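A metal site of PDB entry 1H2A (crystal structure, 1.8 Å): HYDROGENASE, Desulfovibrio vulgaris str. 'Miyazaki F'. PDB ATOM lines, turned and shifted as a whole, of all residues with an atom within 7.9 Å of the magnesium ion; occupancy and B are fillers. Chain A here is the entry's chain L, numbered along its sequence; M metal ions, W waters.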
ATOM      1  N   GLU A  62       0.500 -13.329 -21.712  1.00  0.00           N
ATOM      2  CA  GLU A  62       1.602 -13.702 -20.809  1.00  0.00           C
ATOM      3  C   GLU A  62       2.882 -12.861 -21.011  1.00  0.00           C
ATOM      4  O   GLU A  62       3.674 -12.654 -20.089  1.00  0.00           O
ATOM      5  CB  GLU A  62       1.906 -15.191 -21.001  1.00  0.00           C
ATOM      6  CG  GLU A  62       0.719 -16.107 -20.646  1.00  0.00           C
ATOM      7  CD  GLU A  62       0.772 -17.478 -21.314  1.00  0.00           C
ATOM      8  OE1 GLU A  62       1.220 -17.563 -22.488  1.00  0.00           O
ATOM      9  OE2 GLU A  62       0.315 -18.476 -20.688  1.00  0.00           O
ATOM     10  N   GLU A 337       3.246 -28.204 -20.811  1.00  0.00           N
ATOM     11  CA  GLU A 337       2.840 -27.830 -22.150  1.00  0.00           C
ATOM     12  C   GLU A 337       3.906 -27.969 -23.223  1.00  0.00           C
ATOM     13  O   GLU A 337       5.061 -27.579 -23.019  1.00  0.00           O
ATOM     14  CB  GLU A 337       2.323 -26.393 -22.151  1.00  0.00           C
ATOM     15  CG  GLU A 337       1.420 -26.062 -20.973  1.00  0.00           C
ATOM     16  CD  GLU A 337       0.901 -24.660 -21.019  1.00  0.00           C
ATOM     17  OE1 GLU A 337       1.670 -23.728 -20.728  1.00  0.00           O
ATOM     18  OE2 GLU A 337      -0.292 -24.482 -21.348  1.00  0.00           O
ATOM     19  N   TYR A 344       5.564 -21.845 -31.844  1.00  0.00           N
ATOM     20  CA  TYR A 344       6.442 -21.292 -30.799  1.00  0.00           C
ATOM     21  C   TYR A 344       7.854 -21.847 -31.027  1.00  0.00           C
ATOM     22  O   TYR A 344       8.036 -22.954 -31.573  1.00  0.00           O
ATOM     23  CB  TYR A 344       5.942 -21.653 -29.395  1.00  0.00           C
ATOM     24  CG  TYR A 344       4.604 -21.044 -29.051  1.00  0.00           C
ATOM     25  CD1 TYR A 344       4.509 -19.737 -28.618  1.00  0.00           C
ATOM     26  CD2 TYR A 344       3.416 -21.773 -29.215  1.00  0.00           C
ATOM     27  CE1 TYR A 344       3.295 -19.159 -28.343  1.00  0.00           C
ATOM     28  CE2 TYR A 344       2.187 -21.188 -28.945  1.00  0.00           C
ATOM     29  CZ  TYR A 344       2.127 -19.890 -28.516  1.00  0.00           C
ATOM     30  OH  TYR A 344       0.923 -19.292 -28.222  1.00  0.00           O
ATOM     31  N   PRO A 352       4.278 -25.108 -16.150  1.00  0.00           N
ATOM     32  CA  PRO A 352       3.844 -23.718 -15.993  1.00  0.00           C
ATOM     33  C   PRO A 352       4.726 -22.767 -15.176  1.00  0.00           C
ATOM     34  O   PRO A 352       4.820 -21.575 -15.483  1.00  0.00           O
ATOM     35  CB  PRO A 352       2.440 -23.869 -15.426  1.00  0.00           C
ATOM     36  CG  PRO A 352       1.961 -25.097 -16.070  1.00  0.00           C
ATOM     37  CD  PRO A 352       3.146 -26.028 -15.902  1.00  0.00           C
ATOM     38  N   GLN A 356       7.454 -20.698 -21.015  1.00  0.00           N
ATOM     39  CA  GLN A 356       7.865 -19.618 -21.916  1.00  0.00           C
ATOM     40  C   GLN A 356       6.952 -19.490 -23.110  1.00  0.00           C
ATOM     41  O   GLN A 356       6.533 -20.495 -23.651  1.00  0.00           O
ATOM     42  CB  GLN A 356       9.317 -19.815 -22.377  1.00  0.00           C
ATOM     43  CG  GLN A 356       9.606 -21.134 -23.085  1.00  0.00           C
ATOM     44  CD  GLN A 356      11.110 -21.401 -23.207  1.00  0.00           C
ATOM     45  OE1 GLN A 356      11.936 -20.613 -22.745  1.00  0.00           O
ATOM     46  NE2 GLN A 356      11.452 -22.517 -23.822  1.00  0.00           N
ATOM     47  N   THR A 357       6.644 -18.254 -23.490  1.00  0.00           N
ATOM     48  CA  THR A 357       5.782 -17.936 -24.645  1.00  0.00           C
ATOM     49  C   THR A 357       6.626 -17.173 -25.665  1.00  0.00           C
ATOM     50  O   THR A 357       6.775 -15.941 -25.595  1.00  0.00           O
ATOM     51  CB  THR A 357       4.594 -17.064 -24.187  1.00  0.00           C
ATOM     52  OG1 THR A 357       3.898 -17.751 -23.141  1.00  0.00           O
ATOM     53  CG2 THR A 357       3.633 -16.801 -25.332  1.00  0.00           C
ATOM     54  N   TRP A 372      -1.788 -21.944 -32.640  1.00  0.00           N
ATOM     55  CA  TRP A 372      -1.238 -21.009 -31.692  1.00  0.00           C
ATOM     56  C   TRP A 372      -1.434 -21.500 -30.270  1.00  0.00           C
ATOM     57  O   TRP A 372      -1.236 -20.732 -29.323  1.00  0.00           O
ATOM     58  CB  TRP A 372      -1.864 -19.622 -31.838  1.00  0.00           C
ATOM     59  CG  TRP A 372      -1.294 -18.768 -32.965  1.00  0.00           C
ATOM     60  CD1 TRP A 372      -1.971 -18.286 -34.047  1.00  0.00           C
ATOM     61  CD2 TRP A 372       0.050 -18.253 -33.087  1.00  0.00           C
ATOM     62  NE1 TRP A 372      -1.153 -17.513 -34.832  1.00  0.00           N
ATOM     63  CE2 TRP A 372       0.091 -17.466 -34.259  1.00  0.00           C
ATOM     64  CE3 TRP A 372       1.222 -18.374 -32.319  1.00  0.00           C
ATOM     65  CZ2 TRP A 372       1.268 -16.803 -34.704  1.00  0.00           C
ATOM     66  CZ3 TRP A 372       2.395 -17.716 -32.751  1.00  0.00           C
ATOM     67  CH2 TRP A 372       2.401 -16.938 -33.933  1.00  0.00           C
ATOM     68  N   LYS A 374      -0.561 -24.267 -27.179  1.00  0.00           N
ATOM     69  CA  LYS A 374       0.445 -25.188 -26.699  1.00  0.00           C
ATOM     70  C   LYS A 374      -0.370 -26.472 -26.466  1.00  0.00           C
ATOM     71  O   LYS A 374      -1.613 -26.449 -26.522  1.00  0.00           O
ATOM     72  CB  LYS A 374       1.033 -24.697 -25.383  1.00  0.00           C
ATOM     73  CG  LYS A 374       1.979 -23.521 -25.555  1.00  0.00           C
ATOM     74  CD  LYS A 374       1.870 -22.490 -24.444  1.00  0.00           C
ATOM     75  CE  LYS A 374       3.170 -22.388 -23.674  1.00  0.00           C
ATOM     76  NZ  LYS A 374       3.191 -21.138 -22.861  1.00  0.00           N
ATOM     77  N   SER A 483      -6.226 -23.077 -14.542  1.00  0.00           N
ATOM     78  CA  SER A 483      -5.197 -22.753 -13.549  1.00  0.00           C
ATOM     79  C   SER A 483      -4.253 -21.638 -13.960  1.00  0.00           C
ATOM     80  O   SER A 483      -3.774 -21.625 -15.095  1.00  0.00           O
ATOM     81  CB  SER A 483      -4.387 -24.011 -13.205  1.00  0.00           C
ATOM     82  OG  SER A 483      -3.715 -24.531 -14.355  1.00  0.00           O
ATOM     83  N   TRP A 485      -0.719 -19.359 -12.946  1.00  0.00           N
ATOM     84  CA  TRP A 485       0.541 -19.545 -12.194  1.00  0.00           C
ATOM     85  C   TRP A 485       1.414 -18.306 -12.206  1.00  0.00           C
ATOM     86  O   TRP A 485       1.727 -17.750 -13.272  1.00  0.00           O
ATOM     87  CB  TRP A 485       1.352 -20.694 -12.791  1.00  0.00           C
ATOM     88  CG  TRP A 485       0.545 -21.885 -13.130  1.00  0.00           C
ATOM     89  CD1 TRP A 485      -0.378 -22.000 -14.136  1.00  0.00           C
ATOM     90  CD2 TRP A 485       0.608 -23.174 -12.504  1.00  0.00           C
ATOM     91  NE1 TRP A 485      -0.864 -23.281 -14.193  1.00  0.00           N
ATOM     92  CE2 TRP A 485      -0.285 -24.024 -13.202  1.00  0.00           C
ATOM     93  CE3 TRP A 485       1.345 -23.700 -11.426  1.00  0.00           C
ATOM     94  CZ2 TRP A 485      -0.451 -25.375 -12.859  1.00  0.00           C
ATOM     95  CZ3 TRP A 485       1.164 -25.045 -11.087  1.00  0.00           C
ATOM     96  CH2 TRP A 485       0.273 -25.858 -11.805  1.00  0.00           C
ATOM     97  N   PHE A 496       4.182 -15.182 -15.599  1.00  0.00           N
ATOM     98  CA  PHE A 496       2.771 -15.485 -15.361  1.00  0.00           C
ATOM     99  C   PHE A 496       2.286 -16.396 -16.491  1.00  0.00           C
ATOM    100  O   PHE A 496       2.410 -16.052 -17.663  1.00  0.00           O
ATOM    101  CB  PHE A 496       1.932 -14.208 -15.299  1.00  0.00           C
ATOM    102  CG  PHE A 496       0.620 -14.362 -14.563  1.00  0.00           C
ATOM    103  CD1 PHE A 496      -0.327 -15.271 -14.990  1.00  0.00           C
ATOM    104  CD2 PHE A 496       0.365 -13.619 -13.421  1.00  0.00           C
ATOM    105  CE1 PHE A 496      -1.536 -15.437 -14.293  1.00  0.00           C
ATOM    106  CE2 PHE A 496      -0.822 -13.770 -12.710  1.00  0.00           C
ATOM    107  CZ  PHE A 496      -1.772 -14.679 -13.146  1.00  0.00           C
ATOM    108  N   GLN A 497       1.768 -17.563 -16.144  1.00  0.00           N
ATOM    109  CA  GLN A 497       1.291 -18.505 -17.151  1.00  0.00           C
ATOM    110  C   GLN A 497      -0.161 -18.946 -16.931  1.00  0.00           C
ATOM    111  O   GLN A 497      -0.587 -19.148 -15.786  1.00  0.00           O
ATOM    112  CB  GLN A 497       2.186 -19.732 -17.155  1.00  0.00           C
ATOM    113  CG  GLN A 497       3.600 -19.412 -17.531  1.00  0.00           C
ATOM    114  CD  GLN A 497       3.723 -19.087 -18.993  1.00  0.00           C
ATOM    115  OE1 GLN A 497       3.228 -19.843 -19.840  1.00  0.00           O
ATOM    116  NE2 GLN A 497       4.392 -17.985 -19.304  1.00  0.00           N
ATOM    117  N   LEU A 498      -0.934 -19.020 -18.009  1.00  0.00           N
ATOM    118  CA  LEU A 498      -2.333 -19.477 -17.948  1.00  0.00           C
ATOM    119  C   LEU A 498      -2.396 -20.795 -18.697  1.00  0.00           C
ATOM    120  O   LEU A 498      -1.816 -20.900 -19.771  1.00  0.00           O
ATOM    121  CB  LEU A 498      -3.286 -18.483 -18.655  1.00  0.00           C
ATOM    122  CG  LEU A 498      -3.486 -17.063 -18.101  1.00  0.00           C
ATOM    123  CD1 LEU A 498      -2.304 -16.160 -18.455  1.00  0.00           C
ATOM    124  CD2 LEU A 498      -4.779 -16.455 -18.660  1.00  0.00           C
ATOM    125  N   VAL A 499      -3.045 -21.803 -18.120  1.00  0.00           N
ATOM    126  CA  VAL A 499      -3.255 -23.101 -18.781  1.00  0.00           C
ATOM    127  C   VAL A 499      -4.770 -23.294 -18.626  1.00  0.00           C
ATOM    128  O   VAL A 499      -5.261 -23.476 -17.520  1.00  0.00           O
ATOM    129  CB  VAL A 499      -2.499 -24.223 -18.075  1.00  0.00           C
ATOM    130  CG1 VAL A 499      -2.642 -25.508 -18.857  1.00  0.00           C
ATOM    131  CG2 VAL A 499      -1.030 -23.849 -17.923  1.00  0.00           C
ATOM    132  N   VAL A 500      -5.501 -23.115 -19.722  1.00  0.00           N
ATOM    133  CA  VAL A 500      -6.973 -23.160 -19.699  1.00  0.00           C
ATOM    134  C   VAL A 500      -7.636 -24.427 -20.235  1.00  0.00           C
ATOM    135  O   VAL A 500      -7.002 -25.230 -20.923  1.00  0.00           O
ATOM    136  CB  VAL A 500      -7.566 -21.924 -20.392  1.00  0.00           C
ATOM    137  CG1 VAL A 500      -6.665 -20.726 -20.203  1.00  0.00           C
ATOM    138  CG2 VAL A 500      -7.783 -22.209 -21.871  1.00  0.00           C
ATOM    139  N   THR A 503      -7.344 -25.428 -23.941  1.00  0.00           N
ATOM    140  CA  THR A 503      -5.980 -25.755 -24.315  1.00  0.00           C
ATOM    141  C   THR A 503      -5.896 -27.277 -24.162  1.00  0.00           C
ATOM    142  O   THR A 503      -5.380 -27.966 -25.033  1.00  0.00           O
ATOM    143  CB  THR A 503      -4.940 -25.084 -23.386  1.00  0.00           C
ATOM    144  OG1 THR A 503      -5.376 -23.768 -23.020  1.00  0.00           O
ATOM    145  CG2 THR A 503      -3.629 -24.944 -24.111  1.00  0.00           C
ATOM    146  N   CYS A 549      -9.778 -18.197 -25.043  1.00  0.00           N
ATOM    147  CA  CYS A 549      -9.346 -18.745 -23.759  1.00  0.00           C
ATOM    148  C   CYS A 549      -8.112 -19.602 -23.998  1.00  0.00           C
ATOM    149  O   CYS A 549      -7.070 -19.354 -23.421  1.00  0.00           O
ATOM    150  CB  CYS A 549     -10.448 -19.641 -23.092  1.00  0.00           C
ATOM    151  SG  CYS A 549     -11.504 -18.768 -21.871  1.00  0.00           S
ATOM    152  N   GLY A 550      -8.215 -20.572 -24.898  1.00  0.00           N
ATOM    153  CA  GLY A 550      -7.106 -21.476 -25.159  1.00  0.00           C
ATOM    154  C   GLY A 550      -5.748 -20.949 -25.595  1.00  0.00           C
ATOM    155  O   GLY A 550      -4.743 -21.640 -25.418  1.00  0.00           O
ATOM    156  N   VAL A 551      -5.702 -19.760 -26.184  1.00  0.00           N
ATOM    157  CA  VAL A 551      -4.418 -19.210 -26.644  1.00  0.00           C
ATOM    158  C   VAL A 551      -3.935 -17.991 -25.832  1.00  0.00           C
ATOM    159  O   VAL A 551      -2.737 -17.852 -25.588  1.00  0.00           O
ATOM    160  CB  VAL A 551      -4.511 -18.820 -28.140  1.00  0.00           C
ATOM    161  CG1 VAL A 551      -3.154 -18.268 -28.648  1.00  0.00           C
ATOM    162  CG2 VAL A 551      -4.965 -20.038 -28.962  1.00  0.00           C
ATOM    163  N   HIS A 552      -4.870 -17.151 -25.394  1.00  0.00           N
ATOM    164  CA  HIS A 552      -4.550 -15.919 -24.650  1.00  0.00           C
ATOM    165  C   HIS A 552      -3.320 -15.209 -25.249  1.00  0.00           C
ATOM    166  O   HIS A 552      -3.367 -14.950 -26.493  1.00  0.00           O
ATOM    167  CB  HIS A 552      -4.400 -16.168 -23.122  1.00  0.00           C
ATOM    168  CG  HIS A 552      -3.758 -17.482 -22.773  1.00  0.00           C
ATOM    169  ND1 HIS A 552      -4.398 -18.707 -22.824  1.00  0.00           N
ATOM    170  CD2 HIS A 552      -2.476 -17.762 -22.431  1.00  0.00           C
ATOM    171  CE1 HIS A 552      -3.490 -19.670 -22.514  1.00  0.00           C
ATOM    172  NE2 HIS A 552      -2.299 -19.137 -22.269  1.00  0.00           N
HETATM  173 MG    MG M   1      -0.554 -20.331 -21.514  1.00  0.00          MG
HETATM  174  O   HOH W   1      -1.134 -22.196 -22.297  1.00  0.00           O
HETATM  175  O   HOH W   2       1.111 -21.292 -20.659  1.00  0.00           O
HETATM  176  O   HOH W   3       0.531 -19.907 -23.246  1.00  0.00           O
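The nearest printed residue that does not touch the magnesium ion is Lys 374 (4.1 Å).
Water W3 is bound to the magnesium ion (2.1 Å).
The magnesium ion is bound by water W2 (2.1 Å).
The magnesium ion is bound by water W1, 2.1 Å away.
The magnesium ion is bound by OE2 of Glu 62 (2.2 Å).
The backbone carbonyl oxygen (O) of Leu 498 binds the magnesium ion (2.2 Å).
The magnesium ion is bound by a ring nitrogen (NE2) of His 552.
OE2 of Glu 62 lies close to OE1 of Gln 497 (3.3 Å).
The side-chain carboxylate (OE1) of Glu 62 is in hydrogen-bond range of the side-chain hydroxyl (OG1) of Thr 357.
The backbone carbonyl oxygen (O) of Cys 549 is in hydrogen-bond range of a ring nitrogen (ND1) of His 552, at 2.8 Å.
Water W3 bridges OE1 of Glu 62 (2.6 Å) and NZ of Lys 374 (3.0 Å).
Water W2 lies within hydrogen-bond range of the side-chain carboxylate (OE1) of Glu 337, the side-chain amide oxygen (OE1) of Gln 497 and the side-chain amino group (NZ) of Lys 374.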
